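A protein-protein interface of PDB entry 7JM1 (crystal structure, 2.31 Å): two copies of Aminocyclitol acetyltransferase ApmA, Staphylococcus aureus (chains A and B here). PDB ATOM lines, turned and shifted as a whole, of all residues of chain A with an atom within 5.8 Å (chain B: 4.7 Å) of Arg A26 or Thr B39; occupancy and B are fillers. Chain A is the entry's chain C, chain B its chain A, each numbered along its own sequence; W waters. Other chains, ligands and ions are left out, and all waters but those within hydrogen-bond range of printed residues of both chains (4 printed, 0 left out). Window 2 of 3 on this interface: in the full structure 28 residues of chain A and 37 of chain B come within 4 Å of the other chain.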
ATOM      1  N   PRO A  24       9.132 -27.649 -20.559  1.00  0.00           N
ATOM      2  CA  PRO A  24      10.440 -27.190 -20.082  1.00  0.00           C
ATOM      3  C   PRO A  24      10.659 -25.707 -20.346  1.00  0.00           C
ATOM      4  O   PRO A  24      10.060 -25.101 -21.238  1.00  0.00           O
ATOM      5  CB  PRO A  24      11.431 -28.053 -20.870  1.00  0.00           C
ATOM      6  CG  PRO A  24      10.689 -28.468 -22.084  1.00  0.00           C
ATOM      7  CD  PRO A  24       9.247 -28.592 -21.685  1.00  0.00           C
ATOM      8  N   THR A  25      11.534 -25.123 -19.531  1.00  0.00           N
ATOM      9  CA  THR A  25      11.904 -23.718 -19.601  1.00  0.00           C
ATOM     10  C   THR A  25      13.382 -23.603 -19.955  1.00  0.00           C
ATOM     11  O   THR A  25      14.137 -24.575 -19.888  1.00  0.00           O
ATOM     12  CB  THR A  25      11.622 -22.995 -18.273  1.00  0.00           C
ATOM     13  OG1 THR A  25      12.515 -23.479 -17.263  1.00  0.00           O
ATOM     14  CG2 THR A  25      10.193 -23.235 -17.813  1.00  0.00           C
ATOM     15  N   ARG A  26      13.790 -22.390 -20.335  1.00  0.00           N
ATOM     16  CA  ARG A  26      15.194 -22.146 -20.658  1.00  0.00           C
ATOM     17  C   ARG A  26      16.096 -22.433 -19.462  1.00  0.00           C
ATOM     18  O   ARG A  26      17.157 -23.053 -19.609  1.00  0.00           O
ATOM     19  CB  ARG A  26      15.379 -20.703 -21.126  1.00  0.00           C
ATOM     20  CG  ARG A  26      14.842 -20.422 -22.510  1.00  0.00           C
ATOM     21  CD  ARG A  26      15.919 -20.616 -23.563  1.00  0.00           C
ATOM     22  NE  ARG A  26      15.442 -20.227 -24.882  1.00  0.00           N
ATOM     23  CZ  ARG A  26      16.235 -19.926 -25.902  1.00  0.00           C
ATOM     24  NH1 ARG A  26      17.551 -19.968 -25.752  1.00  0.00           N
ATOM     25  NH2 ARG A  26      15.711 -19.576 -27.066  1.00  0.00           N
ATOM     26  N   ARG A  27      15.695 -21.987 -18.269  1.00  0.00           N
ATOM     27  CA  ARG A  27      16.504 -22.229 -17.077  1.00  0.00           C
ATOM     28  C   ARG A  27      16.661 -23.721 -16.803  1.00  0.00           C
ATOM     29  O   ARG A  27      17.737 -24.175 -16.398  1.00  0.00           O
ATOM     30  CB  ARG A  27      15.890 -21.526 -15.866  1.00  0.00           C
ATOM     31  CG  ARG A  27      16.728 -20.381 -15.330  1.00  0.00           C
ATOM     32  CD  ARG A  27      16.090 -19.734 -14.113  1.00  0.00           C
ATOM     33  NE  ARG A  27      16.148 -20.585 -12.925  1.00  0.00           N
ATOM     34  CZ  ARG A  27      15.090 -21.149 -12.347  1.00  0.00           C
ATOM     35  NH1 ARG A  27      13.875 -20.959 -12.845  1.00  0.00           N
ATOM     36  NH2 ARG A  27      15.245 -21.904 -11.267  1.00  0.00           N
ATOM     37  N   LEU A  28      15.602 -24.502 -17.028  1.00  0.00           N
ATOM     38  CA  LEU A  28      15.686 -25.939 -16.795  1.00  0.00           C
ATOM     39  C   LEU A  28      16.586 -26.614 -17.823  1.00  0.00           C
ATOM     40  O   LEU A  28      17.358 -27.517 -17.478  1.00  0.00           O
ATOM     41  CB  LEU A  28      14.290 -26.560 -16.809  1.00  0.00           C
ATOM     42  CG  LEU A  28      14.261 -28.090 -16.716  1.00  0.00           C
ATOM     43  CD1 LEU A  28      14.863 -28.564 -15.404  1.00  0.00           C
ATOM     44  CD2 LEU A  28      12.851 -28.621 -16.879  1.00  0.00           C
ATOM     45  N   LEU A  29      16.505 -26.192 -19.088  1.00  0.00           N
ATOM     46  CA  LEU A  29      17.365 -26.776 -20.114  1.00  0.00           C
ATOM     47  C   LEU A  29      18.837 -26.541 -19.797  1.00  0.00           C
ATOM     48  O   LEU A  29      19.651 -27.468 -19.883  1.00  0.00           O
ATOM     49  CB  LEU A  29      17.009 -26.207 -21.487  1.00  0.00           C
ATOM     50  CG  LEU A  29      15.606 -26.560 -21.987  1.00  0.00           C
ATOM     51  CD1 LEU A  29      15.308 -25.870 -23.317  1.00  0.00           C
ATOM     52  CD2 LEU A  29      15.443 -28.071 -22.109  1.00  0.00           C
ATOM     53  N   ARG A  30      19.192 -25.316 -19.403  1.00  0.00           N
ATOM     54  CA  ARG A  30      20.566 -25.033 -19.006  1.00  0.00           C
ATOM     55  C   ARG A  30      20.999 -25.915 -17.839  1.00  0.00           C
ATOM     56  O   ARG A  30      22.160 -26.335 -17.765  1.00  0.00           O
ATOM     57  CB  ARG A  30      20.711 -23.552 -18.644  1.00  0.00           C
ATOM     58  CG  ARG A  30      22.138 -23.116 -18.338  1.00  0.00           C
ATOM     59  CD  ARG A  30      22.253 -21.597 -18.246  1.00  0.00           C
ATOM     60  NE  ARG A  30      21.730 -20.927 -19.437  1.00  0.00           N
ATOM     61  CZ  ARG A  30      22.446 -20.668 -20.527  1.00  0.00           C
ATOM     62  NH1 ARG A  30      23.724 -21.024 -20.587  1.00  0.00           N
ATOM     63  NH2 ARG A  30      21.883 -20.057 -21.561  1.00  0.00           N
ATOM     64  N   ALA A  31      20.078 -26.211 -16.918  1.00  0.00           N
ATOM     65  CA  ALA A  31      20.427 -27.062 -15.782  1.00  0.00           C
ATOM     66  C   ALA A  31      20.541 -28.527 -16.183  1.00  0.00           C
ATOM     67  O   ALA A  31      21.282 -29.283 -15.545  1.00  0.00           O
ATOM     68  CB  ALA A  31      19.398 -26.901 -14.664  1.00  0.00           C
ATOM     69  N   VAL B  20      13.315 -14.300 -29.607  1.00  0.00           N
ATOM     70  CA  VAL B  20      12.535 -14.569 -28.400  1.00  0.00           C
ATOM     71  C   VAL B  20      13.295 -15.558 -27.527  1.00  0.00           C
ATOM     72  O   VAL B  20      13.583 -16.685 -27.947  1.00  0.00           O
ATOM     73  CB  VAL B  20      11.137 -15.102 -28.754  1.00  0.00           C
ATOM     74  CG1 VAL B  20      10.358 -15.441 -27.493  1.00  0.00           C
ATOM     75  CG2 VAL B  20      10.380 -14.079 -29.596  1.00  0.00           C
ATOM     76  N   TRP B  21      13.625 -15.136 -26.311  1.00  0.00           N
ATOM     77  CA  TRP B  21      14.337 -15.974 -25.345  1.00  0.00           C
ATOM     78  C   TRP B  21      13.305 -16.497 -24.352  1.00  0.00           C
ATOM     79  O   TRP B  21      12.998 -15.849 -23.352  1.00  0.00           O
ATOM     80  CB  TRP B  21      15.442 -15.179 -24.655  1.00  0.00           C
ATOM     81  CG  TRP B  21      16.528 -16.024 -24.067  1.00  0.00           C
ATOM     82  CD1 TRP B  21      16.507 -16.666 -22.860  1.00  0.00           C
ATOM     83  CD2 TRP B  21      17.805 -16.312 -24.651  1.00  0.00           C
ATOM     84  NE1 TRP B  21      17.688 -17.339 -22.660  1.00  0.00           N
ATOM     85  CE2 TRP B  21      18.502 -17.138 -23.745  1.00  0.00           C
ATOM     86  CE3 TRP B  21      18.426 -15.950 -25.852  1.00  0.00           C
ATOM     87  CZ2 TRP B  21      19.790 -17.612 -24.002  1.00  0.00           C
ATOM     88  CZ3 TRP B  21      19.702 -16.421 -26.107  1.00  0.00           C
ATOM     89  CH2 TRP B  21      20.370 -17.244 -25.186  1.00  0.00           C
ATOM     90  N   GLY B  22      12.753 -17.671 -24.640  1.00  0.00           N
ATOM     91  CA  GLY B  22      11.758 -18.293 -23.790  1.00  0.00           C
ATOM     92  C   GLY B  22      10.567 -18.784 -24.584  1.00  0.00           C
ATOM     93  O   GLY B  22      10.476 -18.616 -25.799  1.00  0.00           O
ATOM     94  N   HIS B  38      11.628 -14.650 -34.176  1.00  0.00           N
ATOM     95  CA  HIS B  38      11.936 -16.065 -34.249  1.00  0.00           C
ATOM     96  C   HIS B  38      12.431 -16.486 -32.879  1.00  0.00           C
ATOM     97  O   HIS B  38      12.786 -15.648 -32.046  1.00  0.00           O
ATOM     98  CB  HIS B  38      12.984 -16.356 -35.332  1.00  0.00           C
ATOM     99  CG  HIS B  38      12.984 -17.773 -35.815  1.00  0.00           C
ATOM    100  ND1 HIS B  38      13.937 -18.691 -35.428  1.00  0.00           N
ATOM    101  CD2 HIS B  38      12.157 -18.426 -36.665  1.00  0.00           C
ATOM    102  CE1 HIS B  38      13.694 -19.851 -36.014  1.00  0.00           C
ATOM    103  NE2 HIS B  38      12.619 -19.717 -36.770  1.00  0.00           N
ATOM    104  N   THR B  39      12.443 -17.793 -32.649  1.00  0.00           N
ATOM    105  CA  THR B  39      13.051 -18.310 -31.436  1.00  0.00           C
ATOM    106  C   THR B  39      14.545 -17.996 -31.425  1.00  0.00           C
ATOM    107  O   THR B  39      15.236 -18.141 -32.438  1.00  0.00           O
ATOM    108  CB  THR B  39      12.816 -19.815 -31.332  1.00  0.00           C
ATOM    109  OG1 THR B  39      11.409 -20.064 -31.233  1.00  0.00           O
ATOM    110  CG2 THR B  39      13.508 -20.376 -30.103  1.00  0.00           C
ATOM    111  N   ALA B  40      15.040 -17.544 -30.273  1.00  0.00           N
ATOM    112  CA  ALA B  40      16.445 -17.180 -30.137  1.00  0.00           C
ATOM    113  C   ALA B  40      17.331 -18.420 -30.037  1.00  0.00           C
ATOM    114  O   ALA B  40      17.093 -19.307 -29.212  1.00  0.00           O
ATOM    115  CB  ALA B  40      16.643 -16.294 -28.907  1.00  0.00           C
ATOM    116  N   ASP B  41      18.358 -18.481 -30.883  1.00  0.00           N
ATOM    117  CA  ASP B  41      19.404 -19.483 -30.723  1.00  0.00           C
ATOM    118  C   ASP B  41      20.755 -18.784 -30.639  1.00  0.00           C
ATOM    119  O   ASP B  41      21.186 -18.398 -29.549  1.00  0.00           O
ATOM    120  CB  ASP B  41      19.378 -20.498 -31.866  1.00  0.00           C
ATOM    121  CG  ASP B  41      20.354 -21.654 -31.645  1.00  0.00           C
ATOM    122  OD1 ASP B  41      20.920 -21.759 -30.531  1.00  0.00           O
ATOM    123  OD2 ASP B  41      20.561 -22.454 -32.582  1.00  0.00           O
ATOM    124  N   ASP B  57      13.444 -16.010 -17.846  1.00  0.00           N
ATOM    125  CA  ASP B  57      14.169 -16.118 -19.108  1.00  0.00           C
ATOM    126  C   ASP B  57      15.295 -15.098 -19.201  1.00  0.00           C
ATOM    127  O   ASP B  57      16.339 -15.383 -19.802  1.00  0.00           O
ATOM    128  CB  ASP B  57      13.211 -15.932 -20.282  1.00  0.00           C
ATOM    129  CG  ASP B  57      12.203 -17.051 -20.396  1.00  0.00           C
ATOM    130  OD1 ASP B  57      12.559 -18.211 -20.093  1.00  0.00           O
ATOM    131  OD2 ASP B  57      11.052 -16.767 -20.796  1.00  0.00           O
ATOM    132  N   ASP B  60      18.400 -16.211 -17.338  1.00  0.00           N
ATOM    133  CA  ASP B  60      19.075 -17.227 -18.137  1.00  0.00           C
ATOM    134  C   ASP B  60      19.819 -16.600 -19.311  1.00  0.00           C
ATOM    135  O   ASP B  60      20.937 -17.019 -19.641  1.00  0.00           O
ATOM    136  CB  ASP B  60      18.074 -18.259 -18.640  1.00  0.00           C
ATOM    137  CG  ASP B  60      18.735 -19.335 -19.460  1.00  0.00           C
ATOM    138  OD1 ASP B  60      19.266 -20.294 -18.858  1.00  0.00           O
ATOM    139  OD2 ASP B  60      18.746 -19.212 -20.701  1.00  0.00           O
HETATM  140  O   HOH W   1      19.118 -21.293 -22.138  1.00  0.00           O
HETATM  141  O   HOH W   2      13.540 -19.794 -18.057  1.00  0.00           O
HETATM  142  O   HOH W   3      12.604 -20.675 -26.415  1.00  0.00           O
HETATM  143  O   HOH W   4      11.435 -20.616 -20.879  1.00  0.00           O
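Of chain B, only Val B20 (3.7 Å), Trp B21 (3.6 Å), Gly B22 (3.7 Å), Thr B39 (3.8 Å), Ala B40 (2.6 Å), Asp B57 (3.9 Å) and Asp B60 (3.6 Å) come within 4 Å of Arg A26.
Leu A29 touches none of the printed residues of chain B.
Of the printed residues of chain B, Arg A30 touches Asp B60.
Of the printed residues of chain A, Val B20 touches Arg A26.
Printed residues of chain A within 4 Å of Trp B21: Arg A26 (3.6 Å).
Printed residues of chain A within 4 Å of Gly B22: Arg A26 (3.7 Å).
Of chain A, only Arg A26 (3.8 Å) comes within 4 Å of Thr B39.
The nearest printed residue of chain A that does not touch Asp B57 is Thr A25 (5.2 Å).
Among the printed residues, merely in contact across the chains: Arg A26 with Val B20 (3.7 Å), Arg A26 with Trp B21 (3.6 Å), Arg A26 with Gly B22 (3.7 Å), Arg A26 with Thr B39 (3.8 Å), Arg A26 with Asp B57 (3.9 Å), Arg A26 with Asp B60 (3.6 Å) and Arg A27 with Asp B60 (3.8 Å).
The backbone NH (N) of Val B20 lies within hydrogen-bond range of the backbone carbonyl oxygen (O) of His B38, 2.8 Å away.
N of Ala B40 lies within hydrogen-bond range of O of Val B20, 2.9 Å away.
The indole nitrogen (NE1) of Trp B21 sits at hydrogen-bond distance from the side-chain carboxylate (OD2) of Asp B60, 2.9 Å away.
O of Ala B40 lies within hydrogen-bond range of NH2 of Arg A26, 2.6 Å away.
OD1 of Asp B60 lies within salt-bridge range of NE of Arg A30 (2.6 Å).
No position is printed for both chains.
Printed residues of chain B that touch a printed residue of chain A: Val B20, Trp B21, Gly B22, Thr B39, Ala B40, Asp B57 and Asp B60.
Hydrophobic or aromatic side chains of chain B within 4 Å of the printed part of chain A: Trp B21 and Ala B40.
Along chain B the printed residues that touch a printed residue of chain A span positions 20 to 60.
Among the printed residues, 9 pairs touch across the chains.
Water W1 lies within hydrogen-bond range of OD2 of Asp B60 (2.6 Å) and NH2 of Arg A30 (3.1 Å).
Water W2 lies within hydrogen-bond range of OD1 of Asp B57 (2.8 Å), N of Arg A27 (3.1 Å) and N of Arg A26 (3.5 Å).
Water W4 lies within hydrogen-bond range of OD1 of Asp B57 (2.8 Å) and N of Arg A26 (3.0 Å).
Water W3 bridges the backbone carbonyl oxygen (O) of Gly B22 (3.0 Å) and the guanidinium group (NE) of Arg A26 (3.3 Å).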
